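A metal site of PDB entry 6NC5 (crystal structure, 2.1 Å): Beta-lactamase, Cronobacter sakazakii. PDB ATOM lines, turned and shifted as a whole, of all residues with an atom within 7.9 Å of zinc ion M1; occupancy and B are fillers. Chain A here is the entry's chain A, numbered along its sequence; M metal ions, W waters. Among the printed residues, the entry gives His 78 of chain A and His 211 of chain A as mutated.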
ATOM      1  N   PHE A   3      -3.214  18.225 -28.447  1.00  0.00           N
ATOM      2  CA  PHE A   3      -2.159  18.639 -27.526  1.00  0.00           C
ATOM      3  C   PHE A   3      -2.300  20.107 -27.144  1.00  0.00           C
ATOM      4  O   PHE A   3      -1.966  20.492 -26.022  1.00  0.00           O
ATOM      5  CB  PHE A   3      -0.786  18.383 -28.146  1.00  0.00           C
ATOM      6  CG  PHE A   3      -0.482  16.931 -28.369  1.00  0.00           C
ATOM      7  CD1 PHE A   3      -0.766  15.991 -27.394  1.00  0.00           C
ATOM      8  CD2 PHE A   3       0.095  16.508 -29.557  1.00  0.00           C
ATOM      9  CE1 PHE A   3      -0.488  14.652 -27.599  1.00  0.00           C
ATOM     10  CE2 PHE A   3       0.382  15.169 -29.766  1.00  0.00           C
ATOM     11  CZ  PHE A   3       0.093  14.243 -28.783  1.00  0.00           C
ATOM     12  N   TRP A   6      -4.759  20.029 -24.477  1.00  0.00           N
ATOM     13  CA  TRP A   6      -4.145  19.423 -23.306  1.00  0.00           C
ATOM     14  C   TRP A   6      -3.171  20.383 -22.625  1.00  0.00           C
ATOM     15  O   TRP A   6      -2.988  20.307 -21.401  1.00  0.00           O
ATOM     16  CB  TRP A   6      -3.409  18.140 -23.703  1.00  0.00           C
ATOM     17  CG  TRP A   6      -4.299  16.951 -23.912  1.00  0.00           C
ATOM     18  CD1 TRP A   6      -5.660  16.909 -23.766  1.00  0.00           C
ATOM     19  CD2 TRP A   6      -3.903  15.638 -24.312  1.00  0.00           C
ATOM     20  NE1 TRP A   6      -6.130  15.650 -24.045  1.00  0.00           N
ATOM     21  CE2 TRP A   6      -5.069  14.846 -24.380  1.00  0.00           C
ATOM     22  CE3 TRP A   6      -2.668  15.050 -24.611  1.00  0.00           C
ATOM     23  CZ2 TRP A   6      -5.036  13.500 -24.735  1.00  0.00           C
ATOM     24  CZ3 TRP A   6      -2.644  13.704 -24.961  1.00  0.00           C
ATOM     25  CH2 TRP A   6      -3.814  12.948 -25.020  1.00  0.00           C
ATOM     26  N   ASN A  26      -4.286  19.038 -18.793  1.00  0.00           N
ATOM     27  CA  ASN A  26      -4.316  17.582 -18.879  1.00  0.00           C
ATOM     28  C   ASN A  26      -2.935  16.943 -18.992  1.00  0.00           C
ATOM     29  O   ASN A  26      -2.859  15.723 -19.187  1.00  0.00           O
ATOM     30  CB  ASN A  26      -5.180  17.134 -20.070  1.00  0.00           C
ATOM     31  CG  ASN A  26      -5.635  15.696 -19.952  1.00  0.00           C
ATOM     32  OD1 ASN A  26      -6.138  15.280 -18.909  1.00  0.00           O
ATOM     33  ND2 ASN A  26      -5.464  14.928 -21.027  1.00  0.00           N
ATOM     34  N   LEU A  27      -1.863  17.711 -18.884  1.00  0.00           N
ATOM     35  CA  LEU A  27      -0.509  17.157 -18.894  1.00  0.00           C
ATOM     36  C   LEU A  27       0.143  17.505 -17.563  1.00  0.00           C
ATOM     37  O   LEU A  27       0.447  18.677 -17.301  1.00  0.00           O
ATOM     38  CB  LEU A  27       0.296  17.705 -20.074  1.00  0.00           C
ATOM     39  CG  LEU A  27      -0.257  17.327 -21.447  1.00  0.00           C
ATOM     40  CD1 LEU A  27       0.597  17.935 -22.545  1.00  0.00           C
ATOM     41  CD2 LEU A  27      -0.359  15.817 -21.619  1.00  0.00           C
ATOM     42  N   SER A  28       0.350  16.494 -16.725  1.00  0.00           N
ATOM     43  CA  SER A  28       0.771  16.719 -15.353  1.00  0.00           C
ATOM     44  C   SER A  28       2.246  17.080 -15.259  1.00  0.00           C
ATOM     45  O   SER A  28       3.073  16.645 -16.065  1.00  0.00           O
ATOM     46  CB  SER A  28       0.483  15.483 -14.513  1.00  0.00           C
ATOM     47  OG  SER A  28      -0.897  15.168 -14.516  1.00  0.00           O
ATOM     48  N   ASP A  42       8.053  14.748 -14.519  1.00  0.00           N
ATOM     49  CA  ASP A  42       7.526  15.008 -15.854  1.00  0.00           C
ATOM     50  C   ASP A  42       7.522  16.493 -16.182  1.00  0.00           C
ATOM     51  O   ASP A  42       7.562  17.340 -15.297  1.00  0.00           O
ATOM     52  CB  ASP A  42       6.121  14.426 -15.997  1.00  0.00           C
ATOM     53  CG  ASP A  42       6.129  13.011 -16.534  1.00  0.00           C
ATOM     54  OD1 ASP A  42       7.154  12.567 -17.091  1.00  0.00           O
ATOM     55  OD2 ASP A  42       5.092  12.322 -16.410  1.00  0.00           O
ATOM     56  N   SER A  72       8.094   9.770 -16.654  1.00  0.00           N
ATOM     57  CA  SER A  72       7.226   8.587 -16.650  1.00  0.00           C
ATOM     58  C   SER A  72       7.450   7.738 -17.900  1.00  0.00           C
ATOM     59  O   SER A  72       7.866   6.584 -17.800  1.00  0.00           O
ATOM     60  CB  SER A  72       5.759   9.020 -16.545  1.00  0.00           C
ATOM     61  OG  SER A  72       5.427   9.962 -17.545  1.00  0.00           O
ATOM     62  N   HIS A  73       7.184   8.292 -19.082  1.00  0.00           N
ATOM     63  CA  HIS A  73       7.533   7.619 -20.327  1.00  0.00           C
ATOM     64  C   HIS A  73       7.926   8.658 -21.372  1.00  0.00           C
ATOM     65  O   HIS A  73       7.523   9.829 -21.307  1.00  0.00           O
ATOM     66  CB  HIS A  73       6.394   6.707 -20.838  1.00  0.00           C
ATOM     67  CG  HIS A  73       5.181   7.433 -21.349  1.00  0.00           C
ATOM     68  ND1 HIS A  73       4.059   7.633 -20.577  1.00  0.00           N
ATOM     69  CD2 HIS A  73       4.897   7.950 -22.566  1.00  0.00           C
ATOM     70  CE1 HIS A  73       3.147   8.278 -21.290  1.00  0.00           C
ATOM     71  NE2 HIS A  73       3.629   8.481 -22.499  1.00  0.00           N
ATOM     72  N   ARG A  75       7.614  10.047 -24.380  1.00  0.00           N
ATOM     73  CA  ARG A  75       6.904  10.607 -25.512  1.00  0.00           C
ATOM     74  C   ARG A  75       6.712  12.103 -25.287  1.00  0.00           C
ATOM     75  O   ARG A  75       6.877  12.608 -24.180  1.00  0.00           O
ATOM     76  CB  ARG A  75       5.561   9.895 -25.740  1.00  0.00           C
ATOM     77  CG  ARG A  75       5.719   8.627 -26.553  1.00  0.00           C
ATOM     78  CD  ARG A  75       4.396   7.906 -26.704  1.00  0.00           C
ATOM     79  NE  ARG A  75       4.530   6.664 -27.448  1.00  0.00           N
ATOM     80  CZ  ARG A  75       3.604   5.713 -27.502  1.00  0.00           C
ATOM     81  NH1 ARG A  75       2.465   5.873 -26.846  1.00  0.00           N
ATOM     82  NH2 ARG A  75       3.808   4.613 -28.211  1.00  0.00           N
ATOM     83  N   LEU A  76       6.350  12.803 -26.364  1.00  0.00           N
ATOM     84  CA  LEU A  76       6.462  14.249 -26.368  1.00  0.00           C
ATOM     85  C   LEU A  76       5.577  14.921 -25.326  1.00  0.00           C
ATOM     86  O   LEU A  76       5.893  16.019 -24.857  1.00  0.00           O
ATOM     87  CB  LEU A  76       6.140  14.783 -27.766  1.00  0.00           C
ATOM     88  CG  LEU A  76       4.663  14.876 -28.177  1.00  0.00           C
ATOM     89  CD1 LEU A  76       4.556  15.710 -29.453  1.00  0.00           C
ATOM     90  CD2 LEU A  76       4.053  13.508 -28.379  1.00  0.00           C
ATOM     91  N   ASP A  77       4.460  14.296 -24.959  1.00  0.00           N
ATOM     92  CA  ASP A  77       3.541  14.943 -24.020  1.00  0.00           C
ATOM     93  C   ASP A  77       3.985  14.823 -22.570  1.00  0.00           C
ATOM     94  O   ASP A  77       3.270  15.303 -21.681  1.00  0.00           O
ATOM     95  CB  ASP A  77       2.122  14.367 -24.171  1.00  0.00           C
ATOM     96  CG  ASP A  77       2.068  12.862 -24.010  1.00  0.00           C
ATOM     97  OD1 ASP A  77       3.085  12.185 -24.242  1.00  0.00           O
ATOM     98  OD2 ASP A  77       0.988  12.354 -23.630  1.00  0.00           O
ATOM     99  N   HIS A  78       5.139  14.212 -22.312  1.00  0.00           N
ATOM    100  CA  HIS A  78       5.701  14.168 -20.962  1.00  0.00           C
ATOM    101  C   HIS A  78       7.192  14.435 -20.914  1.00  0.00           C
ATOM    102  O   HIS A  78       7.663  14.985 -19.916  1.00  0.00           O
ATOM    103  CB  HIS A  78       5.418  12.802 -20.325  1.00  0.00           C
ATOM    104  CG  HIS A  78       3.984  12.383 -20.411  1.00  0.00           C
ATOM    105  ND1 HIS A  78       3.014  12.876 -19.568  1.00  0.00           N
ATOM    106  CD2 HIS A  78       3.353  11.534 -21.259  1.00  0.00           C
ATOM    107  CE1 HIS A  78       1.846  12.338 -19.883  1.00  0.00           C
ATOM    108  NE2 HIS A  78       2.024  11.528 -20.905  1.00  0.00           N
ATOM    109  N   HIS A 149       2.284   0.594 -21.894  1.00  0.00           N
ATOM    110  CA  HIS A 149       2.087   1.744 -22.765  1.00  0.00           C
ATOM    111  C   HIS A 149       3.348   2.034 -23.564  1.00  0.00           C
ATOM    112  O   HIS A 149       3.282   2.349 -24.761  1.00  0.00           O
ATOM    113  CB  HIS A 149       1.677   2.951 -21.919  1.00  0.00           C
ATOM    114  CG  HIS A 149       1.409   4.191 -22.717  1.00  0.00           C
ATOM    115  ND1 HIS A 149       0.311   4.326 -23.540  1.00  0.00           N
ATOM    116  CD2 HIS A 149       2.098   5.353 -22.811  1.00  0.00           C
ATOM    117  CE1 HIS A 149       0.347   5.526 -24.110  1.00  0.00           C
ATOM    118  NE2 HIS A 149       1.419   6.159 -23.678  1.00  0.00           N
ATOM    119  N   ASP A 170       1.818   6.160 -14.359  1.00  0.00           N
ATOM    120  CA  ASP A 170       1.975   6.302 -15.800  1.00  0.00           C
ATOM    121  C   ASP A 170       0.726   5.797 -16.510  1.00  0.00           C
ATOM    122  O   ASP A 170      -0.135   5.132 -15.929  1.00  0.00           O
ATOM    123  CB  ASP A 170       3.212   5.552 -16.274  1.00  0.00           C
ATOM    124  CG  ASP A 170       3.784   6.135 -17.556  1.00  0.00           C
ATOM    125  OD1 ASP A 170       3.014   6.701 -18.355  1.00  0.00           O
ATOM    126  OD2 ASP A 170       5.020   6.030 -17.769  1.00  0.00           O
ATOM    127  N   SER A 171       0.637   6.126 -17.797  1.00  0.00           N
ATOM    128  CA  SER A 171      -0.476   5.656 -18.607  1.00  0.00           C
ATOM    129  C   SER A 171      -0.388   4.147 -18.816  1.00  0.00           C
ATOM    130  O   SER A 171       0.696   3.561 -18.847  1.00  0.00           O
ATOM    131  CB  SER A 171      -0.485   6.365 -19.963  1.00  0.00           C
ATOM    132  OG  SER A 171      -1.199   5.631 -20.935  1.00  0.00           O
ATOM    133  N   ASN A 210      -0.191  11.019 -14.883  1.00  0.00           N
ATOM    134  CA  ASN A 210       0.411  11.989 -15.799  1.00  0.00           C
ATOM    135  C   ASN A 210      -0.605  12.636 -16.741  1.00  0.00           C
ATOM    136  O   ASN A 210      -0.220  13.480 -17.550  1.00  0.00           O
ATOM    137  CB  ASN A 210       1.544  11.339 -16.606  1.00  0.00           C
ATOM    138  CG  ASN A 210       1.106  10.114 -17.377  1.00  0.00           C
ATOM    139  OD1 ASN A 210      -0.077   9.787 -17.451  1.00  0.00           O
ATOM    140  ND2 ASN A 210       2.082   9.420 -17.975  1.00  0.00           N
ATOM    141  N   HIS A 211      -1.882  12.277 -16.639  1.00  0.00           N
ATOM    142  CA  HIS A 211      -2.953  12.942 -17.374  1.00  0.00           C
ATOM    143  C   HIS A 211      -4.048  13.313 -16.385  1.00  0.00           C
ATOM    144  O   HIS A 211      -4.574  12.445 -15.680  1.00  0.00           O
ATOM    145  CB  HIS A 211      -3.501  12.061 -18.494  1.00  0.00           C
ATOM    146  CG  HIS A 211      -2.640  12.043 -19.709  1.00  0.00           C
ATOM    147  ND1 HIS A 211      -2.670  13.040 -20.667  1.00  0.00           N
ATOM    148  CD2 HIS A 211      -1.707  11.160 -20.129  1.00  0.00           C
ATOM    149  CE1 HIS A 211      -1.802  12.763 -21.623  1.00  0.00           C
ATOM    150  NE2 HIS A 211      -1.203  11.625 -21.315  1.00  0.00           N
ATOM    151  N   GLU A 213      -7.179  14.135 -16.495  1.00  0.00           N
ATOM    152  CA  GLU A 213      -8.509  13.548 -16.585  1.00  0.00           C
ATOM    153  C   GLU A 213      -8.615  12.221 -15.866  1.00  0.00           C
ATOM    154  O   GLU A 213      -9.723  11.785 -15.542  1.00  0.00           O
ATOM    155  CB  GLU A 213      -8.889  13.362 -18.052  1.00  0.00           C
ATOM    156  CG  GLU A 213      -8.080  12.287 -18.768  1.00  0.00           C
ATOM    157  CD  GLU A 213      -8.042  12.470 -20.270  1.00  0.00           C
ATOM    158  OE1 GLU A 213      -6.983  12.191 -20.883  1.00  0.00           O
ATOM    159  OE2 GLU A 213      -9.072  12.880 -20.847  1.00  0.00           O
ATOM    160  N   ARG A 214      -7.489  11.563 -15.586  1.00  0.00           N
ATOM    161  CA  ARG A 214      -7.500  10.218 -15.031  1.00  0.00           C
ATOM    162  C   ARG A 214      -7.429  10.185 -13.504  1.00  0.00           C
ATOM    163  O   ARG A 214      -7.620   9.122 -12.917  1.00  0.00           O
ATOM    164  CB  ARG A 214      -6.345   9.393 -15.612  1.00  0.00           C
ATOM    165  CG  ARG A 214      -6.630   8.872 -17.014  1.00  0.00           C
ATOM    166  CD  ARG A 214      -5.363   8.450 -17.724  1.00  0.00           C
ATOM    167  NE  ARG A 214      -5.446   8.692 -19.164  1.00  0.00           N
ATOM    168  CZ  ARG A 214      -4.538   8.296 -20.047  1.00  0.00           C
ATOM    169  NH1 ARG A 214      -3.469   7.623 -19.639  1.00  0.00           N
ATOM    170  NH2 ARG A 214      -4.698   8.564 -21.335  1.00  0.00           N
HETATM  171 ZN    ZN M   1       0.556  11.092 -22.203  1.00  0.00          ZN
HETATM  172 ZN    ZN M   2       1.758   8.225 -23.654  1.00  0.00          ZN
HETATM  173 ZN    ZN M   3       0.586   9.453 -26.587  1.00  0.00          ZN
HETATM  174  O   HOH W   1       0.189   9.054 -22.465  1.00  0.00           O
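ND1 of His 211 sits at hydrogen-bond distance from O of Asn 26, at 3.1 Å. A ring nitrogen (ND1) of His 73 is in hydrogen-bond range of the side-chain carboxylate (OD1) of Asp 170.
Merely in contact with zinc ion M1: His 73.
OD2 of Asp 77 binds zinc ion M1 (2.0 Å). NE2 of His 78 binds zinc ion M1. Zinc ion M1 is bound by NE2 of His 211 (2.0 Å). Water W1 binds zinc ion M1. Zinc ion M1 has four donor atoms within binding distance.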
